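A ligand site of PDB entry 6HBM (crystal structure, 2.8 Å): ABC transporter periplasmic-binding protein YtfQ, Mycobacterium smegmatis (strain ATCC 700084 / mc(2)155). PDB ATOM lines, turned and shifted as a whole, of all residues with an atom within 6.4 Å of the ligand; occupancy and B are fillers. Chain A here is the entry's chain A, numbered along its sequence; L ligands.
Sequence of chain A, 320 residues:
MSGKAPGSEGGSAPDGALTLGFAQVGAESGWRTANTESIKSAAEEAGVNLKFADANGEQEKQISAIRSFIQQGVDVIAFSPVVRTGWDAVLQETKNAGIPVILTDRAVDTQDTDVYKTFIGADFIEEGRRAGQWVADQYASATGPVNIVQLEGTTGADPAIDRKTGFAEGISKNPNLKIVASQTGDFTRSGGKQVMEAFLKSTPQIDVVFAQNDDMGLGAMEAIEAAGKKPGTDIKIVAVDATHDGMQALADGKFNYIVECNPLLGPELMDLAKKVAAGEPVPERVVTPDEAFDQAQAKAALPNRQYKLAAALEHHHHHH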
ATOM      1  N   VAL A  25     -13.354  -6.270 -15.761  1.00  0.00           N
ATOM      2  CA  VAL A  25     -12.695  -6.474 -14.476  1.00  0.00           C
ATOM      3  C   VAL A  25     -13.199  -7.788 -13.883  1.00  0.00           C
ATOM      4  O   VAL A  25     -12.385  -8.656 -13.564  1.00  0.00           O
ATOM      5  CB  VAL A  25     -12.934  -5.276 -13.521  1.00  0.00           C
ATOM      6  N   GLU A  28     -18.127  -8.145  -9.494  1.00  0.00           N
ATOM      7  CA  GLU A  28     -18.111  -8.000  -8.024  1.00  0.00           C
ATOM      8  C   GLU A  28     -19.230  -7.134  -7.424  1.00  0.00           C
ATOM      9  O   GLU A  28     -19.738  -7.426  -6.341  1.00  0.00           O
ATOM     10  CB  GLU A  28     -16.733  -7.464  -7.546  1.00  0.00           C
ATOM     11  CG  GLU A  28     -16.214  -6.177  -8.182  1.00  0.00           C
ATOM     12  CD  GLU A  28     -15.409  -6.317  -9.463  1.00  0.00           C
ATOM     13  OE1 GLU A  28     -14.934  -7.439  -9.764  1.00  0.00           O
ATOM     14  OE2 GLU A  28     -15.263  -5.290 -10.169  1.00  0.00           O
ATOM     15  N   SER A  29     -19.571  -6.064  -8.113  1.00  0.00           N
ATOM     16  CA  SER A  29     -20.528  -5.079  -7.665  1.00  0.00           C
ATOM     17  C   SER A  29     -21.677  -4.981  -8.627  1.00  0.00           C
ATOM     18  O   SER A  29     -21.547  -5.301  -9.797  1.00  0.00           O
ATOM     19  CB  SER A  29     -19.827  -3.739  -7.607  1.00  0.00           C
ATOM     20  OG  SER A  29     -19.420  -3.381  -8.922  1.00  0.00           O
ATOM     21  N   GLY A  30     -22.773  -4.441  -8.130  1.00  0.00           N
ATOM     22  CA  GLY A  30     -23.971  -4.216  -8.933  1.00  0.00           C
ATOM     23  C   GLY A  30     -23.670  -3.256 -10.056  1.00  0.00           C
ATOM     24  O   GLY A  30     -24.225  -3.384 -11.156  1.00  0.00           O
ATOM     25  N   TRP A  31     -22.757  -2.311  -9.786  1.00  0.00           N
ATOM     26  CA  TRP A  31     -22.266  -1.349 -10.759  1.00  0.00           C
ATOM     27  C   TRP A  31     -21.601  -2.085 -11.926  1.00  0.00           C
ATOM     28  O   TRP A  31     -21.760  -1.664 -13.082  1.00  0.00           O
ATOM     29  CB  TRP A  31     -21.269  -0.374 -10.087  1.00  0.00           C
ATOM     30  CG  TRP A  31     -20.902   0.801 -10.949  1.00  0.00           C
ATOM     31  CD1 TRP A  31     -21.395   2.067 -10.872  1.00  0.00           C
ATOM     32  CD2 TRP A  31     -19.929   0.810 -11.987  1.00  0.00           C
ATOM     33  NE1 TRP A  31     -20.798   2.865 -11.818  1.00  0.00           N
ATOM     34  CE2 TRP A  31     -19.864   2.123 -12.503  1.00  0.00           C
ATOM     35  CE3 TRP A  31     -19.080  -0.173 -12.532  1.00  0.00           C
ATOM     36  CZ2 TRP A  31     -19.032   2.472 -13.563  1.00  0.00           C
ATOM     37  CZ3 TRP A  31     -18.255   0.183 -13.590  1.00  0.00           C
ATOM     38  CH2 TRP A  31     -18.262   1.472 -14.112  1.00  0.00           C
ATOM     39  N   ARG A  32     -20.809  -3.151 -11.628  1.00  0.00           N
ATOM     40  CA  ARG A  32     -20.130  -3.965 -12.651  1.00  0.00           C
ATOM     41  C   ARG A  32     -21.104  -4.685 -13.595  1.00  0.00           C
ATOM     42  O   ARG A  32     -20.880  -4.758 -14.815  1.00  0.00           O
ATOM     43  CB  ARG A  32     -19.246  -5.043 -12.012  1.00  0.00           C
ATOM     44  CG  ARG A  32     -17.802  -4.688 -11.909  1.00  0.00           C
ATOM     45  CD  ARG A  32     -17.086  -4.890 -13.215  1.00  0.00           C
ATOM     46  NE  ARG A  32     -16.746  -3.635 -13.881  1.00  0.00           N
ATOM     47  CZ  ARG A  32     -15.813  -2.775 -13.471  1.00  0.00           C
ATOM     48  NH1 ARG A  32     -15.561  -1.675 -14.179  1.00  0.00           N
ATOM     49  NH2 ARG A  32     -15.145  -2.989 -12.343  1.00  0.00           N
ATOM     50  N   SER A  80     -11.152  -2.338 -19.105  1.00  0.00           N
ATOM     51  CA  SER A  80     -11.250  -1.691 -17.803  1.00  0.00           C
ATOM     52  C   SER A  80     -10.130  -2.301 -16.920  1.00  0.00           C
ATOM     53  O   SER A  80     -10.264  -3.447 -16.461  1.00  0.00           O
ATOM     54  CB  SER A  80     -12.635  -1.940 -17.211  1.00  0.00           C
ATOM     55  OG  SER A  80     -12.776  -1.324 -15.937  1.00  0.00           O
ATOM     56  N   ASP A 105     -13.651   3.556 -17.316  1.00  0.00           N
ATOM     57  CA  ASP A 105     -13.722   3.931 -15.887  1.00  0.00           C
ATOM     58  C   ASP A 105     -12.391   3.925 -15.109  1.00  0.00           C
ATOM     59  O   ASP A 105     -12.030   4.990 -14.601  1.00  0.00           O
ATOM     60  CB  ASP A 105     -14.793   3.132 -15.095  1.00  0.00           C
ATOM     61  CG  ASP A 105     -14.516   1.668 -14.808  1.00  0.00           C
ATOM     62  OD1 ASP A 105     -13.718   1.062 -15.525  1.00  0.00           O
ATOM     63  OD2 ASP A 105     -15.135   1.124 -13.876  1.00  0.00           O
ATOM     64  N   ARG A 106     -11.641   2.790 -15.019  1.00  0.00           N
ATOM     65  CA  ARG A 106     -10.377   2.699 -14.305  1.00  0.00           C
ATOM     66  C   ARG A 106      -9.202   3.118 -15.194  1.00  0.00           C
ATOM     67  O   ARG A 106      -9.199   2.795 -16.378  1.00  0.00           O
ATOM     68  CB  ARG A 106     -10.168   1.284 -13.764  1.00  0.00           C
ATOM     69  CG  ARG A 106     -11.350   0.819 -12.928  1.00  0.00           C
ATOM     70  CD  ARG A 106     -11.058  -0.393 -12.085  1.00  0.00           C
ATOM     71  NE  ARG A 106     -12.239  -0.806 -11.314  1.00  0.00           N
ATOM     72  CZ  ARG A 106     -12.259  -1.851 -10.495  1.00  0.00           C
ATOM     73  NH1 ARG A 106     -13.375  -2.152  -9.834  1.00  0.00           N
ATOM     74  NH2 ARG A 106     -11.179  -2.602 -10.320  1.00  0.00           N
ATOM     75  N   PHE A 124     -13.330  10.017  -9.587  1.00  0.00           N
ATOM     76  CA  PHE A 124     -13.335   9.328  -8.309  1.00  0.00           C
ATOM     77  C   PHE A 124     -12.893  10.209  -7.151  1.00  0.00           C
ATOM     78  O   PHE A 124     -13.452  10.091  -6.055  1.00  0.00           O
ATOM     79  CB  PHE A 124     -12.455   8.082  -8.407  1.00  0.00           C
ATOM     80  CG  PHE A 124     -12.823   7.160  -9.532  1.00  0.00           C
ATOM     81  CD1 PHE A 124     -14.132   6.746  -9.712  1.00  0.00           C
ATOM     82  CD2 PHE A 124     -11.883   6.758 -10.454  1.00  0.00           C
ATOM     83  CE1 PHE A 124     -14.496   5.924 -10.783  1.00  0.00           C
ATOM     84  CE2 PHE A 124     -12.221   5.913 -11.510  1.00  0.00           C
ATOM     85  CZ  PHE A 124     -13.538   5.498 -11.669  1.00  0.00           C
ATOM     86  N   GLU A 127     -15.845  12.205  -6.222  1.00  0.00           N
ATOM     87  CA  GLU A 127     -16.836  11.301  -5.609  1.00  0.00           C
ATOM     88  C   GLU A 127     -16.501  11.115  -4.108  1.00  0.00           C
ATOM     89  O   GLU A 127     -17.391  11.290  -3.256  1.00  0.00           O
ATOM     90  CB  GLU A 127     -16.900   9.954  -6.341  1.00  0.00           C
ATOM     91  CG  GLU A 127     -17.584  10.070  -7.687  1.00  0.00           C
ATOM     92  CD  GLU A 127     -17.590   8.817  -8.537  1.00  0.00           C
ATOM     93  OE1 GLU A 127     -17.002   7.795  -8.098  1.00  0.00           O
ATOM     94  OE2 GLU A 127     -18.182   8.852  -9.636  1.00  0.00           O
ATOM     95  N   ALA A 157      -6.665  -0.811  -7.724  1.00  0.00           N
ATOM     96  CA  ALA A 157      -7.610  -0.197  -8.676  1.00  0.00           C
ATOM     97  C   ALA A 157      -7.646   1.334  -8.520  1.00  0.00           C
ATOM     98  O   ALA A 157      -7.612   1.817  -7.373  1.00  0.00           O
ATOM     99  CB  ALA A 157      -9.006  -0.763  -8.438  1.00  0.00           C
ATOM    100  N   PRO A 159     -10.181   3.629  -8.787  1.00  0.00           N
ATOM    101  CA  PRO A 159     -11.202   4.181  -7.864  1.00  0.00           C
ATOM    102  C   PRO A 159     -10.866   4.086  -6.378  1.00  0.00           C
ATOM    103  O   PRO A 159     -11.109   5.048  -5.664  1.00  0.00           O
ATOM    104  CB  PRO A 159     -12.481   3.388  -8.224  1.00  0.00           C
ATOM    105  CG  PRO A 159     -12.007   2.185  -8.963  1.00  0.00           C
ATOM    106  CD  PRO A 159     -10.787   2.654  -9.706  1.00  0.00           C
ATOM    107  N   ARG A 163     -10.544   7.495  -4.472  1.00  0.00           N
ATOM    108  CA  ARG A 163     -11.638   7.770  -3.521  1.00  0.00           C
ATOM    109  C   ARG A 163     -11.141   8.027  -2.122  1.00  0.00           C
ATOM    110  O   ARG A 163     -11.642   8.928  -1.448  1.00  0.00           O
ATOM    111  CB  ARG A 163     -12.675   6.642  -3.510  1.00  0.00           C
ATOM    112  CG  ARG A 163     -13.576   6.718  -4.719  1.00  0.00           C
ATOM    113  CD  ARG A 163     -14.368   5.466  -5.042  1.00  0.00           C
ATOM    114  NE  ARG A 163     -15.234   5.683  -6.189  1.00  0.00           N
ATOM    115  CZ  ARG A 163     -16.027   4.775  -6.737  1.00  0.00           C
ATOM    116  NH1 ARG A 163     -16.078   3.539  -6.242  1.00  0.00           N
ATOM    117  NH2 ARG A 163     -16.778   5.070  -7.795  1.00  0.00           N
ATOM    118  N   ASP A 186     -12.358  -5.434  -1.153  1.00  0.00           N
ATOM    119  CA  ASP A 186     -12.409  -5.880  -2.547  1.00  0.00           C
ATOM    120  C   ASP A 186     -13.701  -5.517  -3.388  1.00  0.00           C
ATOM    121  O   ASP A 186     -13.913  -6.127  -4.453  1.00  0.00           O
ATOM    122  CB  ASP A 186     -12.159  -7.400  -2.592  1.00  0.00           C
ATOM    123  CG  ASP A 186     -11.169  -7.820  -3.658  1.00  0.00           C
ATOM    124  OD1 ASP A 186     -11.536  -7.818  -4.870  1.00  0.00           O
ATOM    125  OD2 ASP A 186     -10.008  -8.143  -3.304  1.00  0.00           O
ATOM    126  N   PHE A 187     -14.481  -4.480  -2.977  1.00  0.00           N
ATOM    127  CA  PHE A 187     -15.722  -4.056  -3.645  1.00  0.00           C
ATOM    128  C   PHE A 187     -16.774  -5.174  -3.708  1.00  0.00           C
ATOM    129  O   PHE A 187     -17.421  -5.331  -4.730  1.00  0.00           O
ATOM    130  CB  PHE A 187     -15.477  -3.491  -5.061  1.00  0.00           C
ATOM    131  CG  PHE A 187     -14.771  -2.170  -5.229  1.00  0.00           C
ATOM    132  CD1 PHE A 187     -15.035  -1.104  -4.376  1.00  0.00           C
ATOM    133  CD2 PHE A 187     -13.986  -1.917  -6.346  1.00  0.00           C
ATOM    134  CE1 PHE A 187     -14.468   0.139  -4.579  1.00  0.00           C
ATOM    135  CE2 PHE A 187     -13.405  -0.675  -6.548  1.00  0.00           C
ATOM    136  CZ  PHE A 187     -13.654   0.341  -5.670  1.00  0.00           C
ATOM    137  N   GLN A 212     -16.610   2.659  -0.133  1.00  0.00           N
ATOM    138  CA  GLN A 212     -16.188   3.098  -1.477  1.00  0.00           C
ATOM    139  C   GLN A 212     -17.032   2.503  -2.639  1.00  0.00           C
ATOM    140  O   GLN A 212     -16.813   2.859  -3.797  1.00  0.00           O
ATOM    141  CB  GLN A 212     -14.681   2.853  -1.689  1.00  0.00           C
ATOM    142  CG  GLN A 212     -13.807   3.856  -0.940  1.00  0.00           C
ATOM    143  CD  GLN A 212     -12.353   3.489  -1.024  1.00  0.00           C
ATOM    144  OE1 GLN A 212     -11.939   2.647  -1.823  1.00  0.00           O
ATOM    145  NE2 GLN A 212     -11.532   4.093  -0.166  1.00  0.00           N
ATOM    146  N   ASN A 213     -18.020   1.668  -2.345  1.00  0.00           N
ATOM    147  CA  ASN A 213     -18.951   1.179  -3.350  1.00  0.00           C
ATOM    148  C   ASN A 213     -20.107   0.655  -2.559  1.00  0.00           C
ATOM    149  O   ASN A 213     -19.884  -0.115  -1.622  1.00  0.00           O
ATOM    150  CB  ASN A 213     -18.276   0.184  -4.309  1.00  0.00           C
ATOM    151  CG  ASN A 213     -18.423  -1.304  -4.094  1.00  0.00           C
ATOM    152  OD1 ASN A 213     -18.263  -1.849  -2.991  1.00  0.00           O
ATOM    153  ND2 ASN A 213     -18.658  -2.023  -5.153  1.00  0.00           N
ATOM    154  N   ASP A 214     -21.309   1.168  -2.793  1.00  0.00           N
ATOM    155  CA  ASP A 214     -22.450   0.783  -1.952  1.00  0.00           C
ATOM    156  C   ASP A 214     -22.518  -0.717  -1.647  1.00  0.00           C
ATOM    157  O   ASP A 214     -22.924  -1.057  -0.554  1.00  0.00           O
ATOM    158  CB  ASP A 214     -23.766   1.313  -2.516  1.00  0.00           C
ATOM    159  CG  ASP A 214     -24.073   0.932  -3.940  1.00  0.00           C
ATOM    160  OD1 ASP A 214     -23.333   0.076  -4.496  1.00  0.00           O
ATOM    161  OD2 ASP A 214     -25.039   1.483  -4.506  1.00  0.00           O
ATOM    162  N   ASP A 215     -22.071  -1.600  -2.569  1.00  0.00           N
ATOM    163  CA  ASP A 215     -22.037  -3.067  -2.371  1.00  0.00           C
ATOM    164  C   ASP A 215     -21.360  -3.465  -1.048  1.00  0.00           C
ATOM    165  O   ASP A 215     -21.919  -4.286  -0.305  1.00  0.00           O
ATOM    166  CB  ASP A 215     -21.371  -3.799  -3.547  1.00  0.00           C
ATOM    167  CG  ASP A 215     -22.341  -4.473  -4.492  1.00  0.00           C
ATOM    168  OD1 ASP A 215     -22.988  -3.750  -5.304  1.00  0.00           O
ATOM    169  OD2 ASP A 215     -22.424  -5.739  -4.460  1.00  0.00           O
ATOM    170  N   VAL A 240     -20.701   5.155  -2.392  1.00  0.00           N
ATOM    171  CA  VAL A 240     -20.612   5.545  -3.811  1.00  0.00           C
ATOM    172  C   VAL A 240     -21.416   4.513  -4.697  1.00  0.00           C
ATOM    173  O   VAL A 240     -21.828   3.463  -4.211  1.00  0.00           O
ATOM    174  CB  VAL A 240     -19.095   5.640  -4.205  1.00  0.00           C
ATOM    175  CG1 VAL A 240     -18.904   6.457  -5.465  1.00  0.00           C
ATOM    176  CG2 VAL A 240     -18.264   6.231  -3.068  1.00  0.00           C
ATOM    177  N   ASP A 241     -21.721   4.902  -5.956  1.00  0.00           N
ATOM    178  CA  ASP A 241     -22.313   4.117  -7.066  1.00  0.00           C
ATOM    179  C   ASP A 241     -23.798   4.410  -7.398  1.00  0.00           C
ATOM    180  O   ASP A 241     -24.120   4.557  -8.577  1.00  0.00           O
ATOM    181  CB  ASP A 241     -22.130   2.594  -6.954  1.00  0.00           C
ATOM    182  CG  ASP A 241     -20.701   2.102  -7.028  1.00  0.00           C
ATOM    183  OD1 ASP A 241     -19.822   2.876  -7.489  1.00  0.00           O
ATOM    184  OD2 ASP A 241     -20.459   0.942  -6.692  1.00  0.00           O
ATOM    185  N   THR A 243     -26.483   2.217  -6.926  1.00  0.00           N
ATOM    186  CA  THR A 243     -27.051   1.027  -7.563  1.00  0.00           C
ATOM    187  C   THR A 243     -28.476   0.840  -7.057  1.00  0.00           C
ATOM    188  O   THR A 243     -28.848   1.472  -6.060  1.00  0.00           O
ATOM    189  CB  THR A 243     -26.193  -0.237  -7.331  1.00  0.00           C
ATOM    190  OG1 THR A 243     -26.280  -0.650  -5.966  1.00  0.00           O
ATOM    191  CG2 THR A 243     -24.738  -0.048  -7.757  1.00  0.00           C
ATOM    192  N   CYS A 261     -22.311   7.182  -9.264  1.00  0.00           N
ATOM    193  CA  CYS A 261     -21.255   6.870 -10.213  1.00  0.00           C
ATOM    194  C   CYS A 261     -21.995   6.238 -11.391  1.00  0.00           C
ATOM    195  O   CYS A 261     -22.671   5.234 -11.195  1.00  0.00           O
ATOM    196  CB  CYS A 261     -20.222   5.925  -9.633  1.00  0.00           C
ATOM    197  SG  CYS A 261     -18.926   5.432 -10.800  1.00  0.00           S
HETATM  198  O1  LIG L   1     -14.367   0.941 -11.417  1.00  0.00           O
HETATM  199  C1  LIG L   1     -15.552   1.429 -10.808  1.00  0.00           C
HETATM  200  C2  LIG L   1     -15.834   0.586  -9.601  1.00  0.00           C
HETATM  201  O2  LIG L   1     -15.789  -0.816  -9.985  1.00  0.00           O
HETATM  202  C3  LIG L   1     -17.195   0.758  -8.969  1.00  0.00           C
HETATM  203  O3  LIG L   1     -17.333   1.888  -8.120  1.00  0.00           O
HETATM  204  C4  LIG L   1     -17.310  -0.544  -8.203  1.00  0.00           C
HETATM  205  O4  LIG L   1     -18.611  -0.757  -7.653  1.00  0.00           O
HETATM  206  C5  LIG L   1     -16.834  -1.534  -9.277  1.00  0.00           C
HETATM  207  O5  LIG L   1     -16.363  -2.803  -8.769  1.00  0.00           O
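OD2 of Asp 105 sits at hydrogen-bond distance from O1 of the ligand (2.6 Å). O4 of the ligand is in hydrogen-bond range of OD2 of Asp 241, 2.7 Å away. The guanidinium group (NE) of Arg 106 sits at hydrogen-bond distance from an oxygen (O1) of the ligand (2.8 Å). O3 of the ligand is in hydrogen-bond range of NH1 of Arg 163 (2.8 Å). An oxygen (O4) of the ligand lies within hydrogen-bond range of the side-chain amide nitrogen (ND2) of Asn 213, at 2.8 Å. O4 of the ligand lies within hydrogen-bond range of OG of Ser 29. The side-chain carboxylate (OE2) of Glu 28 is in hydrogen-bond range of an oxygen (O5) of the ligand. An oxygen (O2) of the ligand is in hydrogen-bond range of the guanidinium group of Arg 32, at 3.3 Å.
Merely in contact with the ligand: Phe 187, Trp 31 and Pro 159. Within 4 Å of the ligand: Glu 28, Ser 29, Trp 31, Arg 32, Asp 105, Arg 106, Pro 159, Arg 163, Phe 187, Asn 213 and Asp 241.
The side-chain carboxylate of Asp 105 lies within salt-bridge range of the guanidinium group of Arg 32 (2.8 Å). OD1 of Asp 105 lies within hydrogen-bond range of OG of Ser 80 (2.6 Å). OD1 of Asp 241 is in salt-bridge range of NH2 of Arg 163 (3.8 Å). O of Asp 241 lies within hydrogen-bond range of N of Cys 261 (3.3 Å). NH1 of Arg 106 lies within salt-bridge range of OE2 of Glu 28, at 3.7 Å. The side-chain sulfur (SG) of Cys 261 lies within hydrogen-bond range of the guanidinium group (NH2) of Arg 163 (3.7 Å). The guanidinium group (NH2) of Arg 163 lies within salt-bridge range of the side-chain carboxylate (OE1) of Glu 127, at 2.8 Å. The backbone NH (N) of Arg 32 is in hydrogen-bond range of the side-chain hydroxyl (OG) of Ser 29 (3.1 Å).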
